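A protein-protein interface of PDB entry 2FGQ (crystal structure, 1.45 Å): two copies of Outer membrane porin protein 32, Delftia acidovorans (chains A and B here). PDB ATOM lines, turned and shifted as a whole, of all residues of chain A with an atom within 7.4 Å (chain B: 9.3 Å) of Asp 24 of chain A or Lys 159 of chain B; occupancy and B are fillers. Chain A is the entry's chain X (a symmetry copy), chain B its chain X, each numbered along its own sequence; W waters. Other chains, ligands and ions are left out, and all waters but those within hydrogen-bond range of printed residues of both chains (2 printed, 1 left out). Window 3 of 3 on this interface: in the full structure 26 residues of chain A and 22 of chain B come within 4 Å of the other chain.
Of the 17 printed residues of chain B, 3 touch a printed residue of chain A.
Hydrophobic or aromatic side chains of chain B that line the printed part of chain A: Phe 156.
Printed residues of chain A that touch a printed residue of chain B: Asp 20, Asp 24, Arg 26 and Tyr 27.
Hydrophobic or aromatic side chains of chain A within 4 Å of the printed part of chain B: Tyr 27.
Among the printed residues, pairs that only touch across the chains: Arg 26 of chain A with Lys 159 of chain B (3.5 Å), Tyr 27 of chain A with Phe 156 of chain B (3.6 Å) and Tyr 27 of chain A with Glu 158 of chain B (3.7 Å).
Water W1 lies within hydrogen-bond range of OH of Tyr 154 of chain B (2.7 Å), OD2 of Asp 157 of chain B (2.7 Å) and OH of Tyr 27 of chain A (3.1 Å).
Water W2 lies within hydrogen-bond range of the backbone carbonyl oxygen of Tyr 27 of chain A (2.8 Å) and the backbone NH of Glu 158 of chain B (2.9 Å).
NH1 of Arg 26 of chain A sits close to O of Glu 158 of chain B (3.4 Å).
The side-chain carboxylate (OD2) of Asp 20 of chain A lies within salt-bridge range of the side-chain amino group (NZ) of Lys 159 of chain B (2.6 Å).
The side-chain amino group (NZ) of Lys 159 of chain B is in salt-bridge range of the side-chain carboxylate (OD2) of Asp 24 of chain A (3.1 Å).
Asp 20 of chain A touches one residue of chain B.
No residue of chain B comes within 4 Å of Ala 22 of chain A.
Gly 23 of chain A touches none of the printed residues of chain B.
Asp 24 of chain A touches one residue of chain B.
No residue of chain B comes within 4 Å of Ser 25 of chain A.
Printed residues of chain B within 4 Å of Arg 26 of chain A: Glu 158 and Lys 159.
Of the printed residues of chain A, Phe 156 of chain B touches Tyr 27 (3.6 Å).
Lys 159 of chain B touches three residues of chain A.
The nearest printed residue of chain A that does not touch Glu 158 of chain B is Val 310 of chain A (4.3 Å).
The backbone NH of Ala 22 of chain A lies within hydrogen-bond range of the side-chain carboxylate of Asp 20 of chain A, at 2.9 Å.
The side-chain carboxylate (OD1) of Asp 157 of chain B sits at hydrogen-bond distance from the backbone NH (N) of Lys 159 of chain B (3.0 Å).
The backbone carbonyl oxygen (O) of Asn 136 of chain B is in hydrogen-bond range of the backbone NH (N) of Phe 156 of chain B, 3.1 Å away.
The backbone carbonyl oxygen (O) of Lys 159 of chain B is in hydrogen-bond range of the side-chain hydroxyl (OG1) of Thr 161 of chain B.
N of Val 17 of chain A lies within hydrogen-bond range of O of Arg 26 of chain A (2.9 Å).
OD1 of Asp 20 of chain A lies within hydrogen-bond range of N of Asp 24 of chain A (3.0 Å).
No position is printed for both chains.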
ATOM      1  N   TYR A  16     -23.422   5.640  27.696  1.00  0.00           N
ATOM      2  CA  TYR A  16     -22.758   4.958  28.777  1.00  0.00           C
ATOM      3  C   TYR A  16     -23.249   5.519  30.100  1.00  0.00           C
ATOM      4  O   TYR A  16     -23.393   6.732  30.260  1.00  0.00           O
ATOM      5  CB  TYR A  16     -21.263   5.212  28.650  1.00  0.00           C
ATOM      6  CG  TYR A  16     -20.427   4.881  29.859  1.00  0.00           C
ATOM      7  CD1 TYR A  16     -20.213   5.818  30.855  1.00  0.00           C
ATOM      8  CD2 TYR A  16     -19.857   3.632  30.002  1.00  0.00           C
ATOM      9  CE1 TYR A  16     -19.425   5.520  31.969  1.00  0.00           C
ATOM     10  CE2 TYR A  16     -19.058   3.321  31.106  1.00  0.00           C
ATOM     11  CZ  TYR A  16     -18.868   4.269  32.080  1.00  0.00           C
ATOM     12  OH  TYR A  16     -18.118   3.975  33.183  1.00  0.00           O
ATOM     13  N   VAL A  17     -23.464   4.629  31.053  1.00  0.00           N
ATOM     14  CA  VAL A  17     -23.575   5.008  32.464  1.00  0.00           C
ATOM     15  C   VAL A  17     -22.604   4.136  33.270  1.00  0.00           C
ATOM     16  O   VAL A  17     -22.339   2.985  32.947  1.00  0.00           O
ATOM     17  CB  VAL A  17     -24.985   4.875  33.045  1.00  0.00           C
ATOM     18  CG1 VAL A  17     -25.953   5.906  32.427  1.00  0.00           C
ATOM     19  CG2 VAL A  17     -25.497   3.447  32.908  1.00  0.00           C
ATOM     20  N   ASN A  18     -22.042   4.715  34.318  1.00  0.00           N
ATOM     21  CA  ASN A  18     -21.042   3.982  35.097  1.00  0.00           C
ATOM     22  C   ASN A  18     -21.618   2.982  36.098  1.00  0.00           C
ATOM     23  O   ASN A  18     -20.937   2.066  36.547  1.00  0.00           O
ATOM     24  CB  ASN A  18     -20.001   4.930  35.709  1.00  0.00           C
ATOM     25  CG  ASN A  18     -20.505   5.801  36.852  1.00  0.00           C
ATOM     26  OD1 ASN A  18     -19.673   6.345  37.663  1.00  0.00           O
ATOM     27  ND2 ASN A  18     -21.779   5.953  36.960  1.00  0.00           N
ATOM     28  N   LYS A  19     -22.880   3.115  36.436  1.00  0.00           N
ATOM     29  CA  LYS A  19     -23.522   2.152  37.320  1.00  0.00           C
ATOM     30  C   LYS A  19     -24.994   1.987  37.014  1.00  0.00           C
ATOM     31  O   LYS A  19     -25.686   2.947  36.630  1.00  0.00           O
ATOM     32  CB  LYS A  19     -23.385   2.526  38.797  1.00  0.00           C
ATOM     33  CG  LYS A  19     -23.288   3.895  39.131  1.00  0.00           C
ATOM     34  CD  LYS A  19     -22.829   4.034  40.609  1.00  0.00           C
ATOM     35  CE  LYS A  19     -21.348   4.363  40.788  1.00  0.00           C
ATOM     36  NZ  LYS A  19     -21.121   5.230  41.999  1.00  0.00           N
ATOM     37  N   ASP A  20     -25.468   0.774  37.246  1.00  0.00           N
ATOM     38  CA  ASP A  20     -26.872   0.429  37.168  1.00  0.00           C
ATOM     39  C   ASP A  20     -27.333   0.012  38.566  1.00  0.00           C
ATOM     40  O   ASP A  20     -26.665   0.334  39.531  1.00  0.00           O
ATOM     41  CB  ASP A  20     -27.082  -0.639  36.101  1.00  0.00           C
ATOM     42  CG  ASP A  20     -26.443  -1.964  36.432  1.00  0.00           C
ATOM     43  OD1 ASP A  20     -25.936  -2.166  37.568  1.00  0.00           O
ATOM     44  OD2 ASP A  20     -26.383  -2.867  35.555  1.00  0.00           O
ATOM     45  N   ALA A  21     -28.448  -0.689  38.680  1.00  0.00           N
ATOM     46  CA  ALA A  21     -29.004  -1.022  40.003  1.00  0.00           C
ATOM     47  C   ALA A  21     -28.137  -1.996  40.796  1.00  0.00           C
ATOM     48  O   ALA A  21     -28.255  -2.075  42.026  1.00  0.00           O
ATOM     49  CB  ALA A  21     -30.420  -1.558  39.863  1.00  0.00           C
ATOM     50  N   ALA A  22     -27.240  -2.689  40.093  1.00  0.00           N
ATOM     51  CA  ALA A  22     -26.254  -3.597  40.685  1.00  0.00           C
ATOM     52  C   ALA A  22     -24.855  -2.991  40.812  1.00  0.00           C
ATOM     53  O   ALA A  22     -23.927  -3.649  41.290  1.00  0.00           O
ATOM     54  CB  ALA A  22     -26.195  -4.839  39.846  1.00  0.00           C
ATOM     55  N   GLY A  23     -24.671  -1.756  40.367  1.00  0.00           N
ATOM     56  CA  GLY A  23     -23.386  -1.091  40.427  1.00  0.00           C
ATOM     57  C   GLY A  23     -22.475  -1.372  39.230  1.00  0.00           C
ATOM     58  O   GLY A  23     -21.310  -0.966  39.253  1.00  0.00           O
ATOM     59  N   ASP A  24     -23.019  -1.992  38.183  1.00  0.00           N
ATOM     60  CA  ASP A  24     -22.259  -2.324  36.957  1.00  0.00           C
ATOM     61  C   ASP A  24     -22.448  -1.257  35.892  1.00  0.00           C
ATOM     62  O   ASP A  24     -23.524  -0.691  35.791  1.00  0.00           O
ATOM     63  CB  ASP A  24     -22.758  -3.636  36.374  1.00  0.00           C
ATOM     64  CG  ASP A  24     -22.566  -4.806  37.316  1.00  0.00           C
ATOM     65  OD1 ASP A  24     -21.539  -4.853  38.019  1.00  0.00           O
ATOM     66  OD2 ASP A  24     -23.402  -5.716  37.413  1.00  0.00           O
ATOM     67  N   SER A  25     -21.410  -0.987  35.110  1.00  0.00           N
ATOM     68  CA  SER A  25     -21.543  -0.046  33.999  1.00  0.00           C
ATOM     69  C   SER A  25     -22.370  -0.650  32.860  1.00  0.00           C
ATOM     70  O   SER A  25     -22.535  -1.870  32.747  1.00  0.00           O
ATOM     71  CB  SER A  25     -20.185   0.425  33.521  1.00  0.00           C
ATOM     72  OG  SER A  25     -19.424  -0.661  33.026  1.00  0.00           O
ATOM     73  N   ARG A  26     -22.905   0.235  32.024  1.00  0.00           N
ATOM     74  CA  ARG A  26     -23.693  -0.158  30.871  1.00  0.00           C
ATOM     75  C   ARG A  26     -23.371   0.750  29.739  1.00  0.00           C
ATOM     76  O   ARG A  26     -23.215   1.937  29.892  1.00  0.00           O
ATOM     77  CB  ARG A  26     -25.191  -0.069  31.183  1.00  0.00           C
ATOM     78  CG  ARG A  26     -26.050  -0.904  30.292  1.00  0.00           C
ATOM     79  CD  ARG A  26     -26.220  -2.341  30.725  1.00  0.00           C
ATOM     80  NE  ARG A  26     -26.851  -2.574  32.019  1.00  0.00           N
ATOM     81  CZ  ARG A  26     -28.130  -2.928  32.223  1.00  0.00           C
ATOM     82  NH1 ARG A  26     -28.994  -3.041  31.231  1.00  0.00           N
ATOM     83  NH2 ARG A  26     -28.547  -3.171  33.442  1.00  0.00           N
ATOM     84  N   TYR A  27     -23.255   0.186  28.567  1.00  0.00           N
ATOM     85  CA  TYR A  27     -23.114   1.035  27.414  1.00  0.00           C
ATOM     86  C   TYR A  27     -23.778   0.399  26.222  1.00  0.00           C
ATOM     87  O   TYR A  27     -24.060  -0.799  26.205  1.00  0.00           O
ATOM     88  CB  TYR A  27     -21.666   1.351  27.185  1.00  0.00           C
ATOM     89  CG  TYR A  27     -20.868   0.126  26.912  1.00  0.00           C
ATOM     90  CD1 TYR A  27     -20.697  -0.307  25.632  1.00  0.00           C
ATOM     91  CD2 TYR A  27     -20.312  -0.617  27.954  1.00  0.00           C
ATOM     92  CE1 TYR A  27     -19.969  -1.452  25.351  1.00  0.00           C
ATOM     93  CE2 TYR A  27     -19.604  -1.816  27.675  1.00  0.00           C
ATOM     94  CZ  TYR A  27     -19.441  -2.209  26.368  1.00  0.00           C
ATOM     95  OH  TYR A  27     -18.727  -3.356  26.029  1.00  0.00           O
ATOM     96  N   VAL A 310     -30.480   2.349  26.500  1.00  0.00           N
ATOM     97  CA  VAL A 310     -29.274   1.753  27.090  1.00  0.00           C
ATOM     98  C   VAL A 310     -29.533   1.360  28.533  1.00  0.00           C
ATOM     99  O   VAL A 310     -29.513   0.179  28.872  1.00  0.00           O
ATOM    100  CB  VAL A 310     -28.019   2.647  26.926  1.00  0.00           C
ATOM    101  CG1 VAL A 310     -26.807   2.015  27.619  1.00  0.00           C
ATOM    102  CG2 VAL A 310     -27.731   2.829  25.447  1.00  0.00           C
ATOM    103  N   TYR A 311     -29.789   2.353  29.379  1.00  0.00           N
ATOM    104  CA  TYR A 311     -30.169   2.080  30.757  1.00  0.00           C
ATOM    105  C   TYR A 311     -30.862   3.327  31.305  1.00  0.00           C
ATOM    106  O   TYR A 311     -30.302   4.420  31.244  1.00  0.00           O
ATOM    107  CB  TYR A 311     -28.956   1.723  31.620  1.00  0.00           C
ATOM    108  CG  TYR A 311     -29.384   1.323  33.029  1.00  0.00           C
ATOM    109  CD1 TYR A 311     -30.046   0.133  33.256  1.00  0.00           C
ATOM    110  CD2 TYR A 311     -29.222   2.206  34.113  1.00  0.00           C
ATOM    111  CE1 TYR A 311     -30.513  -0.198  34.524  1.00  0.00           C
ATOM    112  CE2 TYR A 311     -29.690   1.869  35.408  1.00  0.00           C
ATOM    113  CZ  TYR A 311     -30.329   0.676  35.596  1.00  0.00           C
ATOM    114  OH  TYR A 311     -30.795   0.301  36.838  1.00  0.00           O
ATOM    115  N   GLN A 316     -28.186   2.167  43.189  1.00  0.00           N
ATOM    116  CA  GLN A 316     -28.247   1.880  44.618  1.00  0.00           C
ATOM    117  C   GLN A 316     -28.365   3.184  45.431  1.00  0.00           C
ATOM    118  O   GLN A 316     -27.885   4.249  45.043  1.00  0.00           O
ATOM    119  CB  GLN A 316     -27.016   1.099  45.044  1.00  0.00           C
ATOM    120  CG  GLN A 316     -26.886  -0.224  44.347  1.00  0.00           C
ATOM    121  CD  GLN A 316     -25.448  -0.724  44.293  1.00  0.00           C
ATOM    122  OE1 GLN A 316     -25.155  -1.710  44.926  1.00  0.00           O
ATOM    123  NE2 GLN A 316     -24.557  -0.044  43.533  1.00  0.00           N
ATOM    124  N   GLN A 321     -23.976   8.740  39.936  1.00  0.00           N
ATOM    125  CA  GLN A 321     -23.890   8.115  38.622  1.00  0.00           C
ATOM    126  C   GLN A 321     -23.451   9.154  37.590  1.00  0.00           C
ATOM    127  O   GLN A 321     -23.880  10.295  37.604  1.00  0.00           O
ATOM    128  CB  GLN A 321     -25.254   7.577  38.263  1.00  0.00           C
ATOM    129  CG  GLN A 321     -25.302   6.644  37.064  1.00  0.00           C
ATOM    130  CD  GLN A 321     -26.742   6.448  36.541  1.00  0.00           C
ATOM    131  OE1 GLN A 321     -27.132   5.342  36.096  1.00  0.00           O
ATOM    132  NE2 GLN A 321     -27.509   7.510  36.590  1.00  0.00           N
ATOM    133  N   ASN B 136     -29.104  -2.456  17.977  1.00  0.00           N
ATOM    134  CA  ASN B 136     -27.985  -1.727  18.605  1.00  0.00           C
ATOM    135  C   ASN B 136     -26.731  -1.804  17.764  1.00  0.00           C
ATOM    136  O   ASN B 136     -25.607  -1.811  18.301  1.00  0.00           O
ATOM    137  CB  ASN B 136     -27.679  -2.319  19.971  1.00  0.00           C
ATOM    138  CG  ASN B 136     -28.951  -2.428  20.849  1.00  0.00           C
ATOM    139  OD1 ASN B 136     -29.753  -1.483  20.905  1.00  0.00           O
ATOM    140  ND2 ASN B 136     -29.162  -3.586  21.486  1.00  0.00           N
ATOM    141  N   TYR B 154     -20.583  -3.762  14.523  1.00  0.00           N
ATOM    142  CA  TYR B 154     -20.544  -4.055  15.943  1.00  0.00           C
ATOM    143  C   TYR B 154     -21.944  -3.759  16.489  1.00  0.00           C
ATOM    144  O   TYR B 154     -22.437  -2.693  16.282  1.00  0.00           O
ATOM    145  CB  TYR B 154     -19.514  -3.188  16.706  1.00  0.00           C
ATOM    146  CG  TYR B 154     -19.404  -3.635  18.134  1.00  0.00           C
ATOM    147  CD1 TYR B 154     -18.528  -4.661  18.484  1.00  0.00           C
ATOM    148  CD2 TYR B 154     -20.215  -3.092  19.130  1.00  0.00           C
ATOM    149  CE1 TYR B 154     -18.443  -5.119  19.805  1.00  0.00           C
ATOM    150  CE2 TYR B 154     -20.134  -3.539  20.441  1.00  0.00           C
ATOM    151  CZ  TYR B 154     -19.249  -4.559  20.770  1.00  0.00           C
ATOM    152  OH  TYR B 154     -19.162  -5.020  22.077  1.00  0.00           O
ATOM    153  N   ALA B 155     -22.525  -4.713  17.175  1.00  0.00           N
ATOM    154  CA  ALA B 155     -23.800  -4.483  17.864  1.00  0.00           C
ATOM    155  C   ALA B 155     -23.570  -4.708  19.331  1.00  0.00           C
ATOM    156  O   ALA B 155     -23.065  -5.735  19.744  1.00  0.00           O
ATOM    157  CB  ALA B 155     -24.945  -5.375  17.376  1.00  0.00           C
ATOM    158  N   PHE B 156     -24.007  -3.743  20.121  1.00  0.00           N
ATOM    159  CA  PHE B 156     -23.898  -3.794  21.553  1.00  0.00           C
ATOM    160  C   PHE B 156     -24.902  -4.769  22.192  1.00  0.00           C
ATOM    161  O   PHE B 156     -26.081  -4.781  21.871  1.00  0.00           O
ATOM    162  CB  PHE B 156     -24.166  -2.406  22.143  1.00  0.00           C
ATOM    163  CG  PHE B 156     -23.207  -1.342  21.696  1.00  0.00           C
ATOM    164  CD1 PHE B 156     -23.467  -0.577  20.589  1.00  0.00           C
ATOM    165  CD2 PHE B 156     -22.064  -1.077  22.421  1.00  0.00           C
ATOM    166  CE1 PHE B 156     -22.590   0.416  20.193  1.00  0.00           C
ATOM    167  CE2 PHE B 156     -21.158  -0.078  22.019  1.00  0.00           C
ATOM    168  CZ  PHE B 156     -21.415   0.659  20.906  1.00  0.00           C
ATOM    169  N   ASP B 157     -24.432  -5.538  23.150  1.00  0.00           N
ATOM    170  CA  ASP B 157     -25.274  -6.417  23.932  1.00  0.00           C
ATOM    171  C   ASP B 157     -26.071  -5.718  25.004  1.00  0.00           C
ATOM    172  O   ASP B 157     -27.166  -6.168  25.339  1.00  0.00           O
ATOM    173  CB  ASP B 157     -24.448  -7.526  24.577  1.00  0.00           C
ATOM    174  CG  ASP B 157     -23.269  -7.005  25.315  1.00  0.00           C
ATOM    175  OD1 ASP B 157     -23.333  -6.783  26.566  1.00  0.00           O
ATOM    176  OD2 ASP B 157     -22.219  -6.725  24.704  1.00  0.00           O
ATOM    177  N   GLU B 158     -25.513  -4.648  25.533  1.00  0.00           N
ATOM    178  CA  GLU B 158     -26.185  -3.852  26.574  1.00  0.00           C
ATOM    179  C   GLU B 158     -26.502  -4.686  27.823  1.00  0.00           C
ATOM    180  O   GLU B 158     -27.487  -4.453  28.536  1.00  0.00           O
ATOM    181  CB  GLU B 158     -27.451  -3.171  26.020  1.00  0.00           C
ATOM    182  CG  GLU B 158     -27.080  -2.326  24.829  1.00  0.00           C
ATOM    183  CD  GLU B 158     -28.210  -1.633  24.109  1.00  0.00           C
ATOM    184  OE1 GLU B 158     -29.403  -1.928  24.358  1.00  0.00           O
ATOM    185  OE2 GLU B 158     -27.851  -0.797  23.231  1.00  0.00           O
ATOM    186  N   LYS B 159     -25.661  -5.679  28.051  1.00  0.00           N
ATOM    187  CA  LYS B 159     -25.742  -6.558  29.225  1.00  0.00           C
ATOM    188  C   LYS B 159     -27.029  -7.376  29.260  1.00  0.00           C
ATOM    189  O   LYS B 159     -27.457  -7.826  30.327  1.00  0.00           O
ATOM    190  CB  LYS B 159     -25.515  -5.752  30.531  1.00  0.00           C
ATOM    191  CG  LYS B 159     -24.871  -6.537  31.661  1.00  0.00           C
ATOM    192  CD  LYS B 159     -24.818  -5.699  33.020  1.00  0.00           C
ATOM    193  CE  LYS B 159     -25.996  -5.990  34.014  1.00  0.00           C
ATOM    194  NZ  LYS B 159     -25.855  -5.461  35.511  1.00  0.00           N
ATOM    195  N   GLN B 160     -27.630  -7.612  28.100  1.00  0.00           N
ATOM    196  CA  GLN B 160     -28.762  -8.517  28.020  1.00  0.00           C
ATOM    197  C   GLN B 160     -28.320  -9.882  28.592  1.00  0.00           C
ATOM    198  O   GLN B 160     -27.320 -10.447  28.189  1.00  0.00           O
ATOM    199  CB  GLN B 160     -29.313  -8.696  26.600  1.00  0.00           C
ATOM    200  CG  GLN B 160     -30.503  -9.625  26.612  1.00  0.00           C
ATOM    201  CD  GLN B 160     -31.029 -10.063  25.275  1.00  0.00           C
ATOM    202  OE1 GLN B 160     -31.956 -10.877  25.232  1.00  0.00           O
ATOM    203  NE2 GLN B 160     -30.468  -9.556  24.196  1.00  0.00           N
ATOM    204  N   THR B 161     -29.082 -10.406  29.531  1.00  0.00           N
ATOM    205  CA  THR B 161     -28.704 -11.569  30.283  1.00  0.00           C
ATOM    206  C   THR B 161     -29.747 -12.657  30.175  1.00  0.00           C
ATOM    207  O   THR B 161     -30.937 -12.442  30.444  1.00  0.00           O
ATOM    208  CB  THR B 161     -28.476 -11.170  31.733  1.00  0.00           C
ATOM    209  OG1 THR B 161     -27.350 -10.272  31.803  1.00  0.00           O
ATOM    210  CG2 THR B 161     -28.061 -12.357  32.610  1.00  0.00           C
ATOM    211  N   ILE B 162     -29.297 -13.842  29.766  1.00  0.00           N
ATOM    212  CA  ILE B 162     -30.109 -15.050  29.749  1.00  0.00           C
ATOM    213  C   ILE B 162     -29.234 -16.135  30.357  1.00  0.00           C
ATOM    214  O   ILE B 162     -28.200 -16.538  29.787  1.00  0.00           O
ATOM    215  CB  ILE B 162     -30.585 -15.460  28.345  1.00  0.00           C
ATOM    216  CG1 ILE B 162     -31.399 -14.334  27.677  1.00  0.00           C
ATOM    217  CG2 ILE B 162     -31.438 -16.743  28.382  1.00  0.00           C
ATOM    218  CD1 ILE B 162     -31.794 -14.686  26.233  1.00  0.00           C
ATOM    219  N   GLY B 163     -29.660 -16.633  31.514  1.00  0.00           N
ATOM    220  CA  GLY B 163     -28.905 -17.657  32.201  1.00  0.00           C
ATOM    221  C   GLY B 163     -27.479 -17.198  32.457  1.00  0.00           C
ATOM    222  O   GLY B 163     -27.278 -16.109  32.990  1.00  0.00           O
ATOM    223  N   ALA B 165     -25.274 -16.287  30.226  1.00  0.00           N
ATOM    224  CA  ALA B 165     -24.832 -15.333  29.212  1.00  0.00           C
ATOM    225  C   ALA B 165     -25.249 -13.922  29.621  1.00  0.00           C
ATOM    226  O   ALA B 165     -26.427 -13.685  29.794  1.00  0.00           O
ATOM    227  CB  ALA B 165     -25.449 -15.673  27.890  1.00  0.00           C
ATOM    228  N   ASP B 166     -24.278 -13.024  29.803  1.00  0.00           N
ATOM    229  CA  ASP B 166     -24.539 -11.624  30.155  1.00  0.00           C
ATOM    230  C   ASP B 166     -24.165 -10.645  29.056  1.00  0.00           C
ATOM    231  O   ASP B 166     -24.052  -9.435  29.290  1.00  0.00           O
ATOM    232  CB  ASP B 166     -23.893 -11.246  31.482  1.00  0.00           C
ATOM    233  CG  ASP B 166     -22.390 -11.238  31.454  1.00  0.00           C
ATOM    234  OD1 ASP B 166     -21.771 -11.652  30.442  1.00  0.00           O
ATOM    235  OD2 ASP B 166     -21.761 -10.792  32.460  1.00  0.00           O
ATOM    236  N   SER B 167     -24.047 -11.154  27.834  1.00  0.00           N
ATOM    237  CA  SER B 167     -23.785 -10.308  26.674  1.00  0.00           C
ATOM    238  C   SER B 167     -24.575 -10.769  25.456  1.00  0.00           C
ATOM    239  O   SER B 167     -24.126 -10.633  24.305  1.00  0.00           O
ATOM    240  CB  SER B 167     -22.282 -10.200  26.380  1.00  0.00           C
ATOM    241  OG  SER B 167     -21.676 -11.455  26.104  1.00  0.00           O
ATOM    242  N   VAL B 168     -25.784 -11.252  25.707  1.00  0.00           N
ATOM    243  CA  VAL B 168     -26.640 -11.768  24.641  1.00  0.00           C
ATOM    244  C   VAL B 168     -26.906 -10.667  23.611  1.00  0.00           C
ATOM    245  O   VAL B 168     -27.207  -9.534  23.986  1.00  0.00           O
ATOM    246  CB  VAL B 168     -27.971 -12.331  25.171  1.00  0.00           C
ATOM    247  CG1 VAL B 168     -28.850 -12.822  24.040  1.00  0.00           C
ATOM    248  CG2 VAL B 168     -27.719 -13.472  26.137  1.00  0.00           C
ATOM    249  N   GLY B 169     -26.767 -11.000  22.328  1.00  0.00           N
ATOM    250  CA  GLY B 169     -27.053 -10.088  21.246  1.00  0.00           C
ATOM    251  C   GLY B 169     -25.865  -9.351  20.683  1.00  0.00           C
ATOM    252  O   GLY B 169     -25.967  -8.695  19.648  1.00  0.00           O
ATOM    253  N   ARG B 170     -24.715  -9.441  21.331  1.00  0.00           N
ATOM    254  CA  ARG B 170     -23.520  -8.841  20.772  1.00  0.00           C
ATOM    255  C   ARG B 170     -23.252  -9.436  19.393  1.00  0.00           C
ATOM    256  O   ARG B 170     -23.393 -10.629  19.201  1.00  0.00           O
ATOM    257  CB  ARG B 170     -22.324  -9.062  21.694  1.00  0.00           C
ATOM    258  CG  ARG B 170     -21.086  -8.296  21.276  1.00  0.00           C
ATOM    259  CD  ARG B 170     -19.873  -8.630  22.050  1.00  0.00           C
ATOM    260  NE  ARG B 170     -20.035  -8.226  23.423  1.00  0.00           N
ATOM    261  CZ  ARG B 170     -19.249  -8.607  24.423  1.00  0.00           C
ATOM    262  NH1 ARG B 170     -18.251  -9.462  24.206  1.00  0.00           N
ATOM    263  NH2 ARG B 170     -19.469  -8.117  25.647  1.00  0.00           N
HETATM  264  O   HOH W   1     -20.885  -4.477  24.049  1.00  0.00           O
HETATM  265  O   HOH W   2     -22.980  -3.249  25.517  1.00  0.00           O
